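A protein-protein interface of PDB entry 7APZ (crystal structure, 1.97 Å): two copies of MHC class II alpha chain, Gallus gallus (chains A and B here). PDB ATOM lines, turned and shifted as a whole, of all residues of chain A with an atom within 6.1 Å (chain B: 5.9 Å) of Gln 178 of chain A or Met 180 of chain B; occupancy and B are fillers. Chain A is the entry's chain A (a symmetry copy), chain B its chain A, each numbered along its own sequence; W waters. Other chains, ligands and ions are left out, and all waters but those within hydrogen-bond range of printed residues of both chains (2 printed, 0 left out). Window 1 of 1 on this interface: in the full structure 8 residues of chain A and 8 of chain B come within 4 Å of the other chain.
The side-chain amide oxygen (OE1) of Gln 178 of chain B lies close to the side-chain amide oxygen (OE1) of Gln 178 of chain A.
The side-chain sulfur (SD) of Met 180 of chain A lies within hydrogen-bond range of the backbone NH (N) of Gln 178 of chain B (3.6 Å).
SD of Met 180 of chain B is in hydrogen-bond range of N of Gln 178 of chain A (3.6 Å).
NH1 of Arg 179 of chain A sits close to NH1 of Arg 179 of chain B (3.2 Å).
Water W1 lies within hydrogen-bond range of the backbone NH (N) of Met 180 of chain A (2.8 Å) and the backbone carbonyl oxygen (O) of Gln 178 of chain B (2.8 Å).
Water W2 lies within hydrogen-bond range of N of Met 180 of chain B (2.8 Å) and O of Gln 178 of chain A (2.8 Å).
Hydrophobic or aromatic side chains of chain B that line the printed part of chain A: Met 180.
Printed residues of chain A that touch a printed residue of chain B: Pro 90, Pro 176, Gln 178, Arg 179 and Met 180.
Along chain A the printed residues that touch a printed residue of chain B span positions 90 to 180.
Among the printed residues, 6 pairs touch across the chains.
Among the printed residues, no Asp or Glu carboxylate lies within 4 Å of a Lys or Arg side-chain nitrogen of the other chain.
Among the printed residues, merely in contact across the chains: Pro 176 of chain A with Met 180 of chain B (3.5 Å) and Pro 90 of chain A with Glu 182 of chain B (3.8 Å).
The backbone carbonyl oxygen (O) of Arg 179 of chain B lies within hydrogen-bond range of the backbone NH (N) of Cys 166 of chain B (3.1 Å).
The guanidinium group of Arg 179 of chain A sits at hydrogen-bond distance from the backbone carbonyl oxygen of Leu 92 of chain A.
O of Arg 179 of chain A is in hydrogen-bond range of N of Cys 166 of chain A (3.1 Å).
Gln 178 of chain A touches two residues of chain B.
Printed residues of chain A within 4 Å of Met 180 of chain B: Pro 176 (3.5 Å) and Gln 178 (3.6 Å).
Printed residues of chain A within 4 Å of Gln 178 of chain B: Gln 178 (3.4 Å) and Met 180 (3.6 Å).
Of the printed residues of chain A, Arg 179 of chain B touches Arg 179 (3.1 Å).
Of the printed residues of chain A, Glu 182 of chain B touches Pro 90 (3.8 Å).
Printed residues of chain B within 4 Å of Pro 90 of chain A: Glu 182.
Ala 167 of chain A touches none of the printed residues of chain B.
The nearest residue of chain B that does not touch Gln 178 of chain A is Arg 179 of chain B (4.1 Å).
Gln 178 of chain B touches its own counterpart, Gln 178 of chain A.
Gln 178 of chain A touches Met 180 of chain B, and with the chains exchanged Met 180 of chain A touches Gln 178 of chain B.
Arg 179 of chain A touches its own counterpart, Arg 179 of chain B.
Of the 6 pairs that touch across the chains among the printed residues, 4 have their exchanged pair printed and touching as well.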
ATOM      1  N   PRO A  90       5.997  -1.809 -17.684  1.00  0.00           N
ATOM      2  CA  PRO A  90       5.615  -1.798 -19.099  1.00  0.00           C
ATOM      3  C   PRO A  90       4.236  -2.409 -19.400  1.00  0.00           C
ATOM      4  O   PRO A  90       3.925  -3.453 -18.915  1.00  0.00           O
ATOM      5  CB  PRO A  90       6.690  -2.661 -19.794  1.00  0.00           C
ATOM      6  CG  PRO A  90       7.824  -2.772 -18.809  1.00  0.00           C
ATOM      7  CD  PRO A  90       7.217  -2.586 -17.431  1.00  0.00           C
ATOM      8  N   LEU A  92       2.409  -4.056 -22.724  1.00  0.00           N
ATOM      9  CA  LEU A  92       2.853  -4.698 -23.991  1.00  0.00           C
ATOM     10  C   LEU A  92       1.732  -4.727 -25.020  1.00  0.00           C
ATOM     11  O   LEU A  92       0.606  -5.043 -24.651  1.00  0.00           O
ATOM     12  CB  LEU A  92       3.305  -6.132 -23.724  1.00  0.00           C
ATOM     13  CG  LEU A  92       4.483  -6.288 -22.771  1.00  0.00           C
ATOM     14  CD1 LEU A  92       5.104  -7.677 -22.926  1.00  0.00           C
ATOM     15  CD2 LEU A  92       5.537  -5.202 -22.978  1.00  0.00           C
ATOM     16  N   ARG A 125      10.144 -15.993 -27.671  1.00  0.00           N
ATOM     17  CA  ARG A 125       9.984 -17.464 -27.671  1.00  0.00           C
ATOM     18  C   ARG A 125       9.019 -17.858 -28.782  1.00  0.00           C
ATOM     19  O   ARG A 125       8.131 -17.044 -29.109  1.00  0.00           O
ATOM     20  CB  ARG A 125       9.479 -17.947 -26.311  1.00  0.00           C
ATOM     21  CG  ARG A 125      10.515 -17.887 -25.202  1.00  0.00           C
ATOM     22  CD  ARG A 125       9.987 -18.494 -23.905  1.00  0.00           C
ATOM     23  NE  ARG A 125      10.969 -18.245 -22.861  1.00  0.00           N
ATOM     24  CZ  ARG A 125      11.938 -19.079 -22.470  1.00  0.00           C
ATOM     25  NH1 ARG A 125      12.066 -20.289 -22.986  1.00  0.00           N
ATOM     26  NH2 ARG A 125      12.778 -18.688 -21.529  1.00  0.00           N
ATOM     27  N   SER A 165       5.727 -15.617 -28.083  1.00  0.00           N
ATOM     28  CA  SER A 165       5.668 -14.743 -26.892  1.00  0.00           C
ATOM     29  C   SER A 165       6.801 -13.716 -26.954  1.00  0.00           C
ATOM     30  O   SER A 165       7.874 -14.006 -27.488  1.00  0.00           O
ATOM     31  CB  SER A 165       5.659 -15.540 -25.627  1.00  0.00           C
ATOM     32  OG  SER A 165       6.926 -16.105 -25.365  1.00  0.00           O
ATOM     33  N   CYS A 166       6.512 -12.540 -26.440  1.00  0.00           N
ATOM     34  CA  CYS A 166       7.487 -11.499 -26.091  1.00  0.00           C
ATOM     35  C   CYS A 166       7.395 -11.293 -24.580  1.00  0.00           C
ATOM     36  O   CYS A 166       6.272 -11.105 -24.085  1.00  0.00           O
ATOM     37  CB  CYS A 166       7.158 -10.247 -26.887  1.00  0.00           C
ATOM     38  SG  CYS A 166       8.114  -8.809 -26.356  1.00  0.00           S
ATOM     39  N   ALA A 167       8.523 -11.406 -23.880  1.00  0.00           N
ATOM     40  CA  ALA A 167       8.674 -11.137 -22.435  1.00  0.00           C
ATOM     41  C   ALA A 167       9.579  -9.913 -22.260  1.00  0.00           C
ATOM     42  O   ALA A 167      10.650  -9.846 -22.899  1.00  0.00           O
ATOM     43  CB  ALA A 167       9.210 -12.355 -21.720  1.00  0.00           C
ATOM     44  N   VAL A 168       9.124  -8.947 -21.459  1.00  0.00           N
ATOM     45  CA  VAL A 168       9.899  -7.718 -21.133  1.00  0.00           C
ATOM     46  C   VAL A 168      10.315  -7.773 -19.673  1.00  0.00           C
ATOM     47  O   VAL A 168       9.418  -7.802 -18.818  1.00  0.00           O
ATOM     48  CB  VAL A 168       9.097  -6.447 -21.470  1.00  0.00           C
ATOM     49  CG1 VAL A 168       9.832  -5.175 -21.083  1.00  0.00           C
ATOM     50  CG2 VAL A 168       8.780  -6.454 -22.949  1.00  0.00           C
ATOM     51  N   PRO A 176       9.166 -10.989 -15.523  1.00  0.00           N
ATOM     52  CA  PRO A 176       8.849 -10.287 -16.765  1.00  0.00           C
ATOM     53  C   PRO A 176       7.340 -10.083 -16.960  1.00  0.00           C
ATOM     54  O   PRO A 176       6.544 -10.881 -16.498  1.00  0.00           O
ATOM     55  CB  PRO A 176       9.352 -11.246 -17.854  1.00  0.00           C
ATOM     56  CG  PRO A 176       9.167 -12.613 -17.221  1.00  0.00           C
ATOM     57  CD  PRO A 176       9.476 -12.409 -15.745  1.00  0.00           C
ATOM     58  N   VAL A 177       6.986  -9.040 -17.700  1.00  0.00           N
ATOM     59  CA  VAL A 177       5.661  -8.888 -18.345  1.00  0.00           C
ATOM     60  C   VAL A 177       5.702  -9.672 -19.668  1.00  0.00           C
ATOM     61  O   VAL A 177       6.775  -9.726 -20.309  1.00  0.00           O
ATOM     62  CB  VAL A 177       5.344  -7.396 -18.545  1.00  0.00           C
ATOM     63  CG1 VAL A 177       4.164  -7.195 -19.463  1.00  0.00           C
ATOM     64  CG2 VAL A 177       5.086  -6.736 -17.198  1.00  0.00           C
ATOM     65  N   GLN A 178       4.580 -10.274 -20.066  1.00  0.00           N
ATOM     66  CA  GLN A 178       4.553 -11.218 -21.209  1.00  0.00           C
ATOM     67  C   GLN A 178       3.236 -11.098 -21.992  1.00  0.00           C
ATOM     68  O   GLN A 178       2.201 -10.762 -21.381  1.00  0.00           O
ATOM     69  CB  GLN A 178       4.765 -12.632 -20.682  1.00  0.00           C
ATOM     70  CG  GLN A 178       5.318 -13.567 -21.739  1.00  0.00           C
ATOM     71  CD  GLN A 178       5.760 -14.869 -21.119  1.00  0.00           C
ATOM     72  OE1 GLN A 178       5.269 -15.260 -20.064  1.00  0.00           O
ATOM     73  NE2 GLN A 178       6.708 -15.532 -21.765  1.00  0.00           N
ATOM     74  N   ARG A 179       3.294 -11.393 -23.292  1.00  0.00           N
ATOM     75  CA  ARG A 179       2.153 -11.421 -24.232  1.00  0.00           C
ATOM     76  C   ARG A 179       2.414 -12.558 -25.206  1.00  0.00           C
ATOM     77  O   ARG A 179       3.569 -12.740 -25.585  1.00  0.00           O
ATOM     78  CB  ARG A 179       2.033 -10.121 -25.039  1.00  0.00           C
ATOM     79  CG  ARG A 179       1.264  -9.002 -24.365  1.00  0.00           C
ATOM     80  CD  ARG A 179      -0.240  -9.152 -24.435  1.00  0.00           C
ATOM     81  NE  ARG A 179      -0.755  -8.920 -25.775  1.00  0.00           N
ATOM     82  CZ  ARG A 179      -1.501  -7.880 -26.158  1.00  0.00           C
ATOM     83  NH1 ARG A 179      -1.864  -6.933 -25.300  1.00  0.00           N
ATOM     84  NH2 ARG A 179      -1.885  -7.809 -27.422  1.00  0.00           N
ATOM     85  N   MET A 180       1.368 -13.268 -25.609  1.00  0.00           N
ATOM     86  CA  MET A 180       1.460 -14.377 -26.577  1.00  0.00           C
ATOM     87  C   MET A 180       0.688 -13.957 -27.815  1.00  0.00           C
ATOM     88  O   MET A 180      -0.201 -13.140 -27.704  1.00  0.00           O
ATOM     89  CB  MET A 180       0.901 -15.695 -26.012  1.00  0.00           C
ATOM     90  CG  MET A 180       1.913 -16.481 -25.149  1.00  0.00           C
ATOM     91  SD  MET A 180       2.149 -15.743 -23.487  1.00  0.00           S
ATOM     92  CE  MET A 180       3.247 -16.944 -22.726  1.00  0.00           C
ATOM     93  N   LEU B  94      -7.789  -9.053 -20.984  1.00  0.00           N
ATOM     94  CA  LEU B  94      -7.711  -8.817 -19.513  1.00  0.00           C
ATOM     95  C   LEU B  94      -8.077  -7.358 -19.274  1.00  0.00           C
ATOM     96  O   LEU B  94      -7.323  -6.507 -19.739  1.00  0.00           O
ATOM     97  CB  LEU B  94      -6.300  -9.147 -19.023  1.00  0.00           C
ATOM     98  CG  LEU B  94      -6.066  -9.056 -17.520  1.00  0.00           C
ATOM     99  CD1 LEU B  94      -6.985 -10.004 -16.767  1.00  0.00           C
ATOM    100  CD2 LEU B  94      -4.601  -9.366 -17.199  1.00  0.00           C
ATOM    101  N   VAL B 163       0.664  -5.290 -10.056  1.00  0.00           N
ATOM    102  CA  VAL B 163       0.742  -5.983 -11.371  1.00  0.00           C
ATOM    103  C   VAL B 163      -0.085  -7.264 -11.250  1.00  0.00           C
ATOM    104  O   VAL B 163       0.298  -8.131 -10.456  1.00  0.00           O
ATOM    105  CB  VAL B 163       2.201  -6.283 -11.748  1.00  0.00           C
ATOM    106  CG1 VAL B 163       2.278  -7.084 -13.044  1.00  0.00           C
ATOM    107  CG2 VAL B 163       3.016  -4.989 -11.829  1.00  0.00           C
ATOM    108  N   TYR B 164      -1.177  -7.354 -11.998  1.00  0.00           N
ATOM    109  CA  TYR B 164      -2.057  -8.553 -12.036  1.00  0.00           C
ATOM    110  C   TYR B 164      -1.720  -9.353 -13.299  1.00  0.00           C
ATOM    111  O   TYR B 164      -1.332  -8.773 -14.334  1.00  0.00           O
ATOM    112  CB  TYR B 164      -3.528  -8.158 -11.965  1.00  0.00           C
ATOM    113  CG  TYR B 164      -3.924  -7.474 -10.676  1.00  0.00           C
ATOM    114  CD1 TYR B 164      -3.740  -6.114 -10.491  1.00  0.00           C
ATOM    115  CD2 TYR B 164      -4.463  -8.193  -9.629  1.00  0.00           C
ATOM    116  CE1 TYR B 164      -4.114  -5.487  -9.310  1.00  0.00           C
ATOM    117  CE2 TYR B 164      -4.818  -7.590  -8.435  1.00  0.00           C
ATOM    118  CZ  TYR B 164      -4.660  -6.230  -8.276  1.00  0.00           C
ATOM    119  OH  TYR B 164      -5.028  -5.642  -7.101  1.00  0.00           O
ATOM    120  N   SER B 165      -1.800 -10.670 -13.202  1.00  0.00           N
ATOM    121  CA  SER B 165      -1.706 -11.580 -14.363  1.00  0.00           C
ATOM    122  C   SER B 165      -2.825 -12.621 -14.290  1.00  0.00           C
ATOM    123  O   SER B 165      -3.241 -13.012 -13.196  1.00  0.00           O
ATOM    124  CB  SER B 165      -0.343 -12.184 -14.477  1.00  0.00           C
ATOM    125  OG  SER B 165      -0.124 -13.156 -13.477  1.00  0.00           O
ATOM    126  N   CYS B 166      -3.302 -13.004 -15.455  1.00  0.00           N
ATOM    127  CA  CYS B 166      -4.139 -14.189 -15.685  1.00  0.00           C
ATOM    128  C   CYS B 166      -3.345 -15.120 -16.601  1.00  0.00           C
ATOM    129  O   CYS B 166      -2.864 -14.645 -17.642  1.00  0.00           O
ATOM    130  CB  CYS B 166      -5.457 -13.737 -16.289  1.00  0.00           C
ATOM    131  SG  CYS B 166      -6.471 -15.115 -16.869  1.00  0.00           S
ATOM    132  N   GLN B 178      -0.555 -16.115 -21.136  1.00  0.00           N
ATOM    133  CA  GLN B 178      -0.544 -15.155 -20.005  1.00  0.00           C
ATOM    134  C   GLN B 178      -0.734 -13.714 -20.504  1.00  0.00           C
ATOM    135  O   GLN B 178      -0.319 -13.410 -21.640  1.00  0.00           O
ATOM    136  CB  GLN B 178       0.765 -15.314 -19.241  1.00  0.00           C
ATOM    137  CG  GLN B 178       0.658 -14.840 -17.804  1.00  0.00           C
ATOM    138  CD  GLN B 178       1.875 -15.255 -17.015  1.00  0.00           C
ATOM    139  OE1 GLN B 178       2.945 -15.463 -17.577  1.00  0.00           O
ATOM    140  NE2 GLN B 178       1.704 -15.395 -15.708  1.00  0.00           N
ATOM    141  N   ARG B 179      -1.324 -12.869 -19.655  1.00  0.00           N
ATOM    142  CA  ARG B 179      -1.551 -11.426 -19.878  1.00  0.00           C
ATOM    143  C   ARG B 179      -1.376 -10.741 -18.533  1.00  0.00           C
ATOM    144  O   ARG B 179      -1.799 -11.315 -17.532  1.00  0.00           O
ATOM    145  CB  ARG B 179      -2.972 -11.132 -20.380  1.00  0.00           C
ATOM    146  CG  ARG B 179      -3.173 -11.247 -21.878  1.00  0.00           C
ATOM    147  CD  ARG B 179      -2.677 -10.054 -22.665  1.00  0.00           C
ATOM    148  NE  ARG B 179      -3.519  -8.882 -22.478  1.00  0.00           N
ATOM    149  CZ  ARG B 179      -4.310  -8.331 -23.401  1.00  0.00           C
ATOM    150  NH1 ARG B 179      -4.388  -8.823 -24.633  1.00  0.00           N
ATOM    151  NH2 ARG B 179      -5.023  -7.268 -23.069  1.00  0.00           N
ATOM    152  N   MET B 180      -0.798  -9.546 -18.528  1.00  0.00           N
ATOM    153  CA  MET B 180      -0.591  -8.745 -17.306  1.00  0.00           C
ATOM    154  C   MET B 180      -1.437  -7.492 -17.442  1.00  0.00           C
ATOM    155  O   MET B 180      -1.722  -7.094 -18.552  1.00  0.00           O
ATOM    156  CB  MET B 180       0.889  -8.380 -17.090  1.00  0.00           C
ATOM    157  CG  MET B 180       1.709  -9.490 -16.396  1.00  0.00           C
ATOM    158  SD  MET B 180       2.106 -10.883 -17.518  1.00  0.00           S
ATOM    159  CE  MET B 180       3.148 -11.895 -16.462  1.00  0.00           C
ATOM    160  N   TRP B 181      -1.788  -6.897 -16.319  1.00  0.00           N
ATOM    161  CA  TRP B 181      -2.581  -5.660 -16.257  1.00  0.00           C
ATOM    162  C   TRP B 181      -2.146  -4.894 -15.010  1.00  0.00           C
ATOM    163  O   TRP B 181      -1.897  -5.524 -13.960  1.00  0.00           O
ATOM    164  CB  TRP B 181      -4.082  -5.998 -16.304  1.00  0.00           C
ATOM    165  CG  TRP B 181      -4.933  -4.781 -16.237  1.00  0.00           C
ATOM    166  CD1 TRP B 181      -5.428  -4.057 -17.279  1.00  0.00           C
ATOM    167  CD2 TRP B 181      -5.327  -4.105 -15.038  1.00  0.00           C
ATOM    168  NE1 TRP B 181      -6.125  -2.981 -16.803  1.00  0.00           N
ATOM    169  CE2 TRP B 181      -6.090  -2.990 -15.433  1.00  0.00           C
ATOM    170  CE3 TRP B 181      -5.124  -4.345 -13.679  1.00  0.00           C
ATOM    171  CZ2 TRP B 181      -6.636  -2.101 -14.511  1.00  0.00           C
ATOM    172  CZ3 TRP B 181      -5.651  -3.465 -12.767  1.00  0.00           C
ATOM    173  CH2 TRP B 181      -6.419  -2.369 -13.182  1.00  0.00           C
ATOM    174  N   GLU B 182      -2.028  -3.578 -15.145  1.00  0.00           N
ATOM    175  CA  GLU B 182      -1.677  -2.659 -14.040  1.00  0.00           C
ATOM    176  C   GLU B 182      -2.678  -1.522 -14.015  1.00  0.00           C
ATOM    177  O   GLU B 182      -3.057  -1.012 -15.077  1.00  0.00           O
ATOM    178  CB  GLU B 182      -0.295  -2.039 -14.242  1.00  0.00           C
ATOM    179  CG  GLU B 182       0.768  -3.059 -14.580  1.00  0.00           C
ATOM    180  CD  GLU B 182       0.869  -3.363 -16.067  1.00  0.00           C
ATOM    181  OE1 GLU B 182       0.557  -2.457 -16.863  1.00  0.00           O
ATOM    182  OE2 GLU B 182       1.251  -4.504 -16.429  1.00  0.00           O
HETATM  183  O   HOH W   1      -1.129 -12.906 -24.313  1.00  0.00           O
HETATM  184  O   HOH W   2       0.432  -8.596 -20.902  1.00  0.00           O
